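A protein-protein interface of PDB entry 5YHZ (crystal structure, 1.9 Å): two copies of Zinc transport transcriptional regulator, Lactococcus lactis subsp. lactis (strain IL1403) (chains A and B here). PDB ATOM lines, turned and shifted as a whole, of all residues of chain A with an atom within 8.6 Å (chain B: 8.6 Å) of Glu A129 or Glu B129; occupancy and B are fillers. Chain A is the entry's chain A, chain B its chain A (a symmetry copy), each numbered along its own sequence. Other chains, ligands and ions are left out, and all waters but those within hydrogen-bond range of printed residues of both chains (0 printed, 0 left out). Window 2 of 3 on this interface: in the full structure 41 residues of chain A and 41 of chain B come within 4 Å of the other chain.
The side-chain amide nitrogen (NE2) of Gln A131 sits at hydrogen-bond distance from the backbone carbonyl oxygen (O) of Phe A126 (3.2 Å). N of Thr A127 lies within hydrogen-bond range of OE1 of Glu A130, 2.9 Å away. O of Phe B126 sits at hydrogen-bond distance from NE2 of Gln B131. N of Thr B127 sits at hydrogen-bond distance from OE1 of Glu B130 (2.9 Å).
CE1 of Phe A126 touches O of Val B133, at 3.9 Å. Glu A129 touches Glu B129. Val B133 touches Glu A130. Phe B126 touches Val A133 (CE1 to O, 3.9 Å). Val A133 touches Glu B130 (CG2 to CG, 3.6 Å). CG1 of Ile B134 touches CG1 of Val A133, at 3.7 Å. Ile A134 touches Val B133.
Of the printed residues of chain B, Glu A129 touches Glu B129. Glu A132 touches none of the printed residues of chain B. Of the printed residues of chain B, Val A133 touches Phe B126, Glu B130 and Ile B134. Printed residues of chain A within 4 Å of Phe B126: Val A133. Asp B128 touches none of the printed residues of chain A. Glu B129 touches just one residue of chain A: Glu A129 (3.9 Å). Of the printed residues of chain A, Glu B130 touches Val A133 (3.6 Å). Printed residues of chain A within 4 Å of Ile B134: Val A133 (3.7 Å). The nearest residue of chain B that does not touch Glu A129 is Val B133 (6.1 Å). The nearest residue of chain A that does not touch Glu B129 is Val A133 (6.1 Å). The nearest printed residue of chain A that does not touch Val B133 is Val A133 (4.2 Å).
Printed residues of chain A that touch a printed residue of chain B: Phe A126, Glu A129, Glu A130, Val A133 and Ile A134. Hydrophobic or aromatic side chains of chain A within 4 Å of the printed part of chain B: Phe A126, Val A133 and Ile A134. Hydrophobic or aromatic side chains of chain B that line the printed part of chain A: Phe B126, Val B133 and Ile B134. Along chain B the printed residues that touch a printed residue of chain A span positions 126 to 134. Among the printed residues, 7 pairs touch across the chains. Among the printed residues, no Asp or Glu carboxylate lies within 4 Å of a Lys or Arg side-chain nitrogen of the other chain.
Phe A126 touches Val B133, and with the chains exchanged Val A133 touches Phe B126. Glu B129 touches its own counterpart, Glu A129. Glu A130 touches Val B133, and with the chains exchanged Val A133 touches Glu B130. Val A133 touches Ile B134, and with the chains exchanged Ile A134 touches Val B133. Of the 7 pairs that touch across the chains among the printed residues, 7 have their exchanged pair printed and touching as well.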
ATOM      1  N   PHE A 126      19.899  23.577 -18.891  1.00  0.00           N
ATOM      2  CA  PHE A 126      18.927  22.637 -18.374  1.00  0.00           C
ATOM      3  C   PHE A 126      17.585  22.735 -19.144  1.00  0.00           C
ATOM      4  O   PHE A 126      17.181  23.800 -19.579  1.00  0.00           O
ATOM      5  CB  PHE A 126      18.701  22.909 -16.907  1.00  0.00           C
ATOM      6  CG  PHE A 126      19.913  22.693 -16.097  1.00  0.00           C
ATOM      7  CD1 PHE A 126      20.257  21.420 -15.666  1.00  0.00           C
ATOM      8  CD2 PHE A 126      20.748  23.768 -15.788  1.00  0.00           C
ATOM      9  CE1 PHE A 126      21.401  21.233 -14.874  1.00  0.00           C
ATOM     10  CE2 PHE A 126      21.903  23.576 -15.003  1.00  0.00           C
ATOM     11  CZ  PHE A 126      22.221  22.306 -14.562  1.00  0.00           C
ATOM     12  N   THR A 127      16.903  21.604 -19.262  1.00  0.00           N
ATOM     13  CA  THR A 127      15.586  21.530 -19.948  1.00  0.00           C
ATOM     14  C   THR A 127      14.576  22.137 -18.999  1.00  0.00           C
ATOM     15  O   THR A 127      14.904  22.398 -17.799  1.00  0.00           O
ATOM     16  CB  THR A 127      15.215  20.049 -20.149  1.00  0.00           C
ATOM     17  OG1 THR A 127      15.222  19.397 -18.897  1.00  0.00           O
ATOM     18  CG2 THR A 127      16.232  19.341 -21.035  1.00  0.00           C
ATOM     19  N   ASP A 128      13.371  22.386 -19.491  1.00  0.00           N
ATOM     20  CA  ASP A 128      12.310  22.926 -18.673  1.00  0.00           C
ATOM     21  C   ASP A 128      12.078  22.148 -17.428  1.00  0.00           C
ATOM     22  O   ASP A 128      11.835  22.718 -16.370  1.00  0.00           O
ATOM     23  CB  ASP A 128      10.986  23.001 -19.431  1.00  0.00           C
ATOM     24  CG  ASP A 128      11.069  23.914 -20.609  1.00  0.00           C
ATOM     25  OD1 ASP A 128      11.811  24.889 -20.483  1.00  0.00           O
ATOM     26  OD2 ASP A 128      10.481  23.633 -21.688  1.00  0.00           O
ATOM     27  N   GLU A 129      12.084  20.845 -17.545  1.00  0.00           N
ATOM     28  CA  GLU A 129      11.753  20.037 -16.428  1.00  0.00           C
ATOM     29  C   GLU A 129      12.869  20.206 -15.371  1.00  0.00           C
ATOM     30  O   GLU A 129      12.606  20.345 -14.177  1.00  0.00           O
ATOM     31  CB  GLU A 129      11.765  18.583 -16.858  1.00  0.00           C
ATOM     32  CG  GLU A 129      11.735  17.644 -15.685  1.00  0.00           C
ATOM     33  CD  GLU A 129      11.441  16.243 -16.167  1.00  0.00           C
ATOM     34  OE1 GLU A 129      12.422  15.503 -16.456  1.00  0.00           O
ATOM     35  OE2 GLU A 129      10.219  15.932 -16.321  1.00  0.00           O
ATOM     36  N   GLU A 130      14.074  20.248 -15.868  1.00  0.00           N
ATOM     37  CA  GLU A 130      15.245  20.461 -14.967  1.00  0.00           C
ATOM     38  C   GLU A 130      15.220  21.834 -14.373  1.00  0.00           C
ATOM     39  O   GLU A 130      15.488  22.005 -13.212  1.00  0.00           O
ATOM     40  CB  GLU A 130      16.529  20.254 -15.775  1.00  0.00           C
ATOM     41  CG  GLU A 130      16.673  18.801 -16.078  1.00  0.00           C
ATOM     42  CD  GLU A 130      17.741  18.565 -17.113  1.00  0.00           C
ATOM     43  OE1 GLU A 130      18.220  19.518 -17.790  1.00  0.00           O
ATOM     44  OE2 GLU A 130      18.092  17.417 -17.247  1.00  0.00           O
ATOM     45  N   GLN A 131      14.844  22.837 -15.155  1.00  0.00           N
ATOM     46  CA  GLN A 131      14.754  24.158 -14.609  1.00  0.00           C
ATOM     47  C   GLN A 131      13.688  24.218 -13.507  1.00  0.00           C
ATOM     48  O   GLN A 131      13.893  24.876 -12.533  1.00  0.00           O
ATOM     49  CB  GLN A 131      14.523  25.213 -15.689  1.00  0.00           C
ATOM     50  CG  GLN A 131      15.665  25.281 -16.700  1.00  0.00           C
ATOM     51  CD  GLN A 131      15.436  26.497 -17.652  1.00  0.00           C
ATOM     52  OE1 GLN A 131      14.423  27.143 -17.539  1.00  0.00           O
ATOM     53  NE2 GLN A 131      16.312  26.721 -18.612  1.00  0.00           N
ATOM     54  N   GLU A 132      12.597  23.466 -13.649  1.00  0.00           N
ATOM     55  CA  GLU A 132      11.536  23.494 -12.622  1.00  0.00           C
ATOM     56  C   GLU A 132      12.131  22.858 -11.361  1.00  0.00           C
ATOM     57  O   GLU A 132      11.892  23.315 -10.261  1.00  0.00           O
ATOM     58  CB  GLU A 132      10.305  22.674 -13.107  1.00  0.00           C
ATOM     59  CG  GLU A 132       9.167  22.598 -12.013  1.00  0.00           C
ATOM     60  CD  GLU A 132       8.192  21.426 -12.264  1.00  0.00           C
ATOM     61  OE1 GLU A 132       8.331  20.719 -13.298  1.00  0.00           O
ATOM     62  OE2 GLU A 132       7.275  21.213 -11.432  1.00  0.00           O
ATOM     63  N   VAL A 133      12.880  21.770 -11.525  1.00  0.00           N
ATOM     64  CA  VAL A 133      13.501  21.136 -10.389  1.00  0.00           C
ATOM     65  C   VAL A 133      14.416  22.096  -9.674  1.00  0.00           C
ATOM     66  O   VAL A 133      14.376  22.224  -8.428  1.00  0.00           O
ATOM     67  CB  VAL A 133      14.357  19.930 -10.816  1.00  0.00           C
ATOM     68  CG1 VAL A 133      15.286  19.483  -9.615  1.00  0.00           C
ATOM     69  CG2 VAL A 133      13.456  18.783 -11.346  1.00  0.00           C
ATOM     70  N   ILE A 134      15.295  22.733 -10.431  1.00  0.00           N
ATOM     71  CA  ILE A 134      16.218  23.674  -9.853  1.00  0.00           C
ATOM     72  C   ILE A 134      15.418  24.820  -9.199  1.00  0.00           C
ATOM     73  O   ILE A 134      15.730  25.233  -8.124  1.00  0.00           O
ATOM     74  CB  ILE A 134      17.152  24.266 -10.945  1.00  0.00           C
ATOM     75  CG1 ILE A 134      18.049  23.171 -11.508  1.00  0.00           C
ATOM     76  CG2 ILE A 134      17.892  25.544 -10.384  1.00  0.00           C
ATOM     77  CD1 ILE A 134      18.832  23.531 -12.895  1.00  0.00           C
ATOM     78  N   SER A 135      14.325  25.241  -9.832  1.00  0.00           N
ATOM     79  CA  SER A 135      13.579  26.402  -9.340  1.00  0.00           C
ATOM     80  C   SER A 135      12.909  25.977  -8.065  1.00  0.00           C
ATOM     81  O   SER A 135      12.917  26.706  -7.133  1.00  0.00           O
ATOM     82  CB  SER A 135      12.462  26.870 -10.335  1.00  0.00           C
ATOM     83  OG  SER A 135      11.704  27.853  -9.650  1.00  0.00           O
ATOM     84  N   LYS A 136      12.444  24.743  -7.997  1.00  0.00           N
ATOM     85  CA  LYS A 136      11.719  24.306  -6.808  1.00  0.00           C
ATOM     86  C   LYS A 136      12.723  24.156  -5.703  1.00  0.00           C
ATOM     87  O   LYS A 136      12.433  24.476  -4.565  1.00  0.00           O
ATOM     88  CB  LYS A 136      11.024  22.957  -7.059  1.00  0.00           C
ATOM     89  CG  LYS A 136       9.787  23.111  -8.017  1.00  0.00           C
ATOM     90  CD  LYS A 136       8.988  21.835  -8.104  1.00  0.00           C
ATOM     91  CE  LYS A 136       8.024  21.660  -6.943  1.00  0.00           C
ATOM     92  NZ  LYS A 136       6.678  22.231  -7.246  1.00  0.00           N
ATOM     93  N   PHE B 126      13.603  15.218  -3.389  1.00  0.00           N
ATOM     94  CA  PHE B 126      13.839  15.042  -4.807  1.00  0.00           C
ATOM     95  C   PHE B 126      14.291  13.594  -5.127  1.00  0.00           C
ATOM     96  O   PHE B 126      14.978  12.958  -4.345  1.00  0.00           O
ATOM     97  CB  PHE B 126      14.891  16.024  -5.263  1.00  0.00           C
ATOM     98  CG  PHE B 126      14.461  17.424  -5.115  1.00  0.00           C
ATOM     99  CD1 PHE B 126      13.675  18.028  -6.087  1.00  0.00           C
ATOM    100  CD2 PHE B 126      14.811  18.147  -3.974  1.00  0.00           C
ATOM    101  CE1 PHE B 126      13.294  19.372  -5.945  1.00  0.00           C
ATOM    102  CE2 PHE B 126      14.416  19.493  -3.828  1.00  0.00           C
ATOM    103  CZ  PHE B 126      13.653  20.087  -4.814  1.00  0.00           C
ATOM    104  N   THR B 127      13.914  13.118  -6.305  1.00  0.00           N
ATOM    105  CA  THR B 127      14.286  11.758  -6.776  1.00  0.00           C
ATOM    106  C   THR B 127      15.742  11.828  -7.179  1.00  0.00           C
ATOM    107  O   THR B 127      16.328  12.953  -7.260  1.00  0.00           O
ATOM    108  CB  THR B 127      13.463  11.429  -8.036  1.00  0.00           C
ATOM    109  OG1 THR B 127      13.685  12.429  -9.008  1.00  0.00           O
ATOM    110  CG2 THR B 127      11.970  11.415  -7.732  1.00  0.00           C
ATOM    111  N   ASP B 128      16.352  10.676  -7.416  1.00  0.00           N
ATOM    112  CA  ASP B 128      17.730  10.616  -7.846  1.00  0.00           C
ATOM    113  C   ASP B 128      18.008  11.465  -9.034  1.00  0.00           C
ATOM    114  O   ASP B 128      19.050  12.107  -9.114  1.00  0.00           O
ATOM    115  CB  ASP B 128      18.163   9.190  -8.179  1.00  0.00           C
ATOM    116  CG  ASP B 128      18.091   8.293  -6.988  1.00  0.00           C
ATOM    117  OD1 ASP B 128      18.338   8.819  -5.901  1.00  0.00           O
ATOM    118  OD2 ASP B 128      17.705   7.098  -7.100  1.00  0.00           O
ATOM    119  N   GLU B 129      17.121  11.432  -9.995  1.00  0.00           N
ATOM    120  CA  GLU B 129      17.373  12.120 -11.209  1.00  0.00           C
ATOM    121  C   GLU B 129      17.368  13.637 -10.906  1.00  0.00           C
ATOM    122  O   GLU B 129      18.219  14.388 -11.381  1.00  0.00           O
ATOM    123  CB  GLU B 129      16.228  11.855 -12.166  1.00  0.00           C
ATOM    124  CG  GLU B 129      16.250  12.782 -13.349  1.00  0.00           C
ATOM    125  CD  GLU B 129      15.290  12.281 -14.402  1.00  0.00           C
ATOM    126  OE1 GLU B 129      14.103  12.708 -14.366  1.00  0.00           O
ATOM    127  OE2 GLU B 129      15.728  11.402 -15.208  1.00  0.00           O
ATOM    128  N   GLU B 130      16.439  14.012 -10.073  1.00  0.00           N
ATOM    129  CA  GLU B 130      16.349  15.441  -9.648  1.00  0.00           C
ATOM    130  C   GLU B 130      17.535  15.828  -8.821  1.00  0.00           C
ATOM    131  O   GLU B 130      18.078  16.889  -8.988  1.00  0.00           O
ATOM    132  CB  GLU B 130      15.057  15.636  -8.850  1.00  0.00           C
ATOM    133  CG  GLU B 130      13.900  15.552  -9.787  1.00  0.00           C
ATOM    134  CD  GLU B 130      12.601  15.435  -9.036  1.00  0.00           C
ATOM    135  OE1 GLU B 130      12.578  15.175  -7.800  1.00  0.00           O
ATOM    136  OE2 GLU B 130      11.602  15.601  -9.695  1.00  0.00           O
ATOM    137  N   GLN B 131      17.989  14.943  -7.944  1.00  0.00           N
ATOM    138  CA  GLN B 131      19.155  15.255  -7.172  1.00  0.00           C
ATOM    139  C   GLN B 131      20.377  15.432  -8.084  1.00  0.00           C
ATOM    140  O   GLN B 131      21.170  16.288  -7.836  1.00  0.00           O
ATOM    141  CB  GLN B 131      19.406  14.230  -6.068  1.00  0.00           C
ATOM    142  CG  GLN B 131      18.267  14.167  -5.054  1.00  0.00           C
ATOM    143  CD  GLN B 131      18.684  13.235  -3.871  1.00  0.00           C
ATOM    144  OE1 GLN B 131      19.741  12.656  -3.931  1.00  0.00           O
ATOM    145  NE2 GLN B 131      17.825  13.037  -2.892  1.00  0.00           N
ATOM    146  N   GLU B 132      20.466  14.663  -9.169  1.00  0.00           N
ATOM    147  CA  GLU B 132      21.627  14.786 -10.074  1.00  0.00           C
ATOM    148  C   GLU B 132      21.521  16.164 -10.736  1.00  0.00           C
ATOM    149  O   GLU B 132      22.510  16.846 -10.918  1.00  0.00           O
ATOM    150  CB  GLU B 132      21.579  13.666 -11.155  1.00  0.00           C
ATOM    151  CG  GLU B 132      22.753  13.797 -12.204  1.00  0.00           C
ATOM    152  CD  GLU B 132      22.452  13.034 -13.514  1.00  0.00           C
ATOM    153  OE1 GLU B 132      21.397  12.352 -13.602  1.00  0.00           O
ATOM    154  OE2 GLU B 132      23.278  13.107 -14.459  1.00  0.00           O
ATOM    155  N   VAL B 133      20.312  16.555 -11.134  1.00  0.00           N
ATOM    156  CA  VAL B 133      20.129  17.853 -11.735  1.00  0.00           C
ATOM    157  C   VAL B 133      20.567  18.945 -10.794  1.00  0.00           C
ATOM    158  O   VAL B 133      21.306  19.878 -11.183  1.00  0.00           O
ATOM    159  CB  VAL B 133      18.649  18.113 -12.070  1.00  0.00           C
ATOM    160  CG1 VAL B 133      18.438  19.648 -12.394  1.00  0.00           C
ATOM    161  CG2 VAL B 133      18.179  17.181 -13.219  1.00  0.00           C
ATOM    162  N   ILE B 134      20.070  18.889  -9.568  1.00  0.00           N
ATOM    163  CA  ILE B 134      20.421  19.881  -8.586  1.00  0.00           C
ATOM    164  C   ILE B 134      21.946  19.834  -8.353  1.00  0.00           C
ATOM    165  O   ILE B 134      22.573  20.846  -8.278  1.00  0.00           O
ATOM    166  CB  ILE B 134      19.693  19.602  -7.242  1.00  0.00           C
ATOM    167  CG1 ILE B 134      18.191  19.778  -7.419  1.00  0.00           C
ATOM    168  CG2 ILE B 134      20.356  20.451  -6.085  1.00  0.00           C
ATOM    169  CD1 ILE B 134      17.254  19.185  -6.221  1.00  0.00           C
ATOM    170  N   SER B 135      22.527  18.636  -8.347  1.00  0.00           N
ATOM    171  CA  SER B 135      23.946  18.497  -8.013  1.00  0.00           C
ATOM    172  C   SER B 135      24.719  19.078  -9.164  1.00  0.00           C
ATOM    173  O   SER B 135      25.651  19.774  -8.945  1.00  0.00           O
ATOM    174  CB  SER B 135      24.386  17.002  -7.848  1.00  0.00           C
ATOM    175  OG  SER B 135      25.799  17.013  -7.731  1.00  0.00           O
ATOM    176  N   LYS B 136      24.246  18.888 -10.381  1.00  0.00           N
ATOM    177  CA  LYS B 136      24.999  19.367 -11.536  1.00  0.00           C
ATOM    178  C   LYS B 136      24.881  20.863 -11.554  1.00  0.00           C
ATOM    179  O   LYS B 136      25.834  21.547 -11.883  1.00  0.00           O
ATOM    180  CB  LYS B 136      24.424  18.789 -12.840  1.00  0.00           C
ATOM    181  CG  LYS B 136      24.754  17.260 -12.992  1.00  0.00           C
ATOM    182  CD  LYS B 136      24.369  16.740 -14.354  1.00  0.00           C
ATOM    183  CE  LYS B 136      25.413  17.035 -15.417  1.00  0.00           C
ATOM    184  NZ  LYS B 136      26.404  15.927 -15.548  1.00  0.00           N
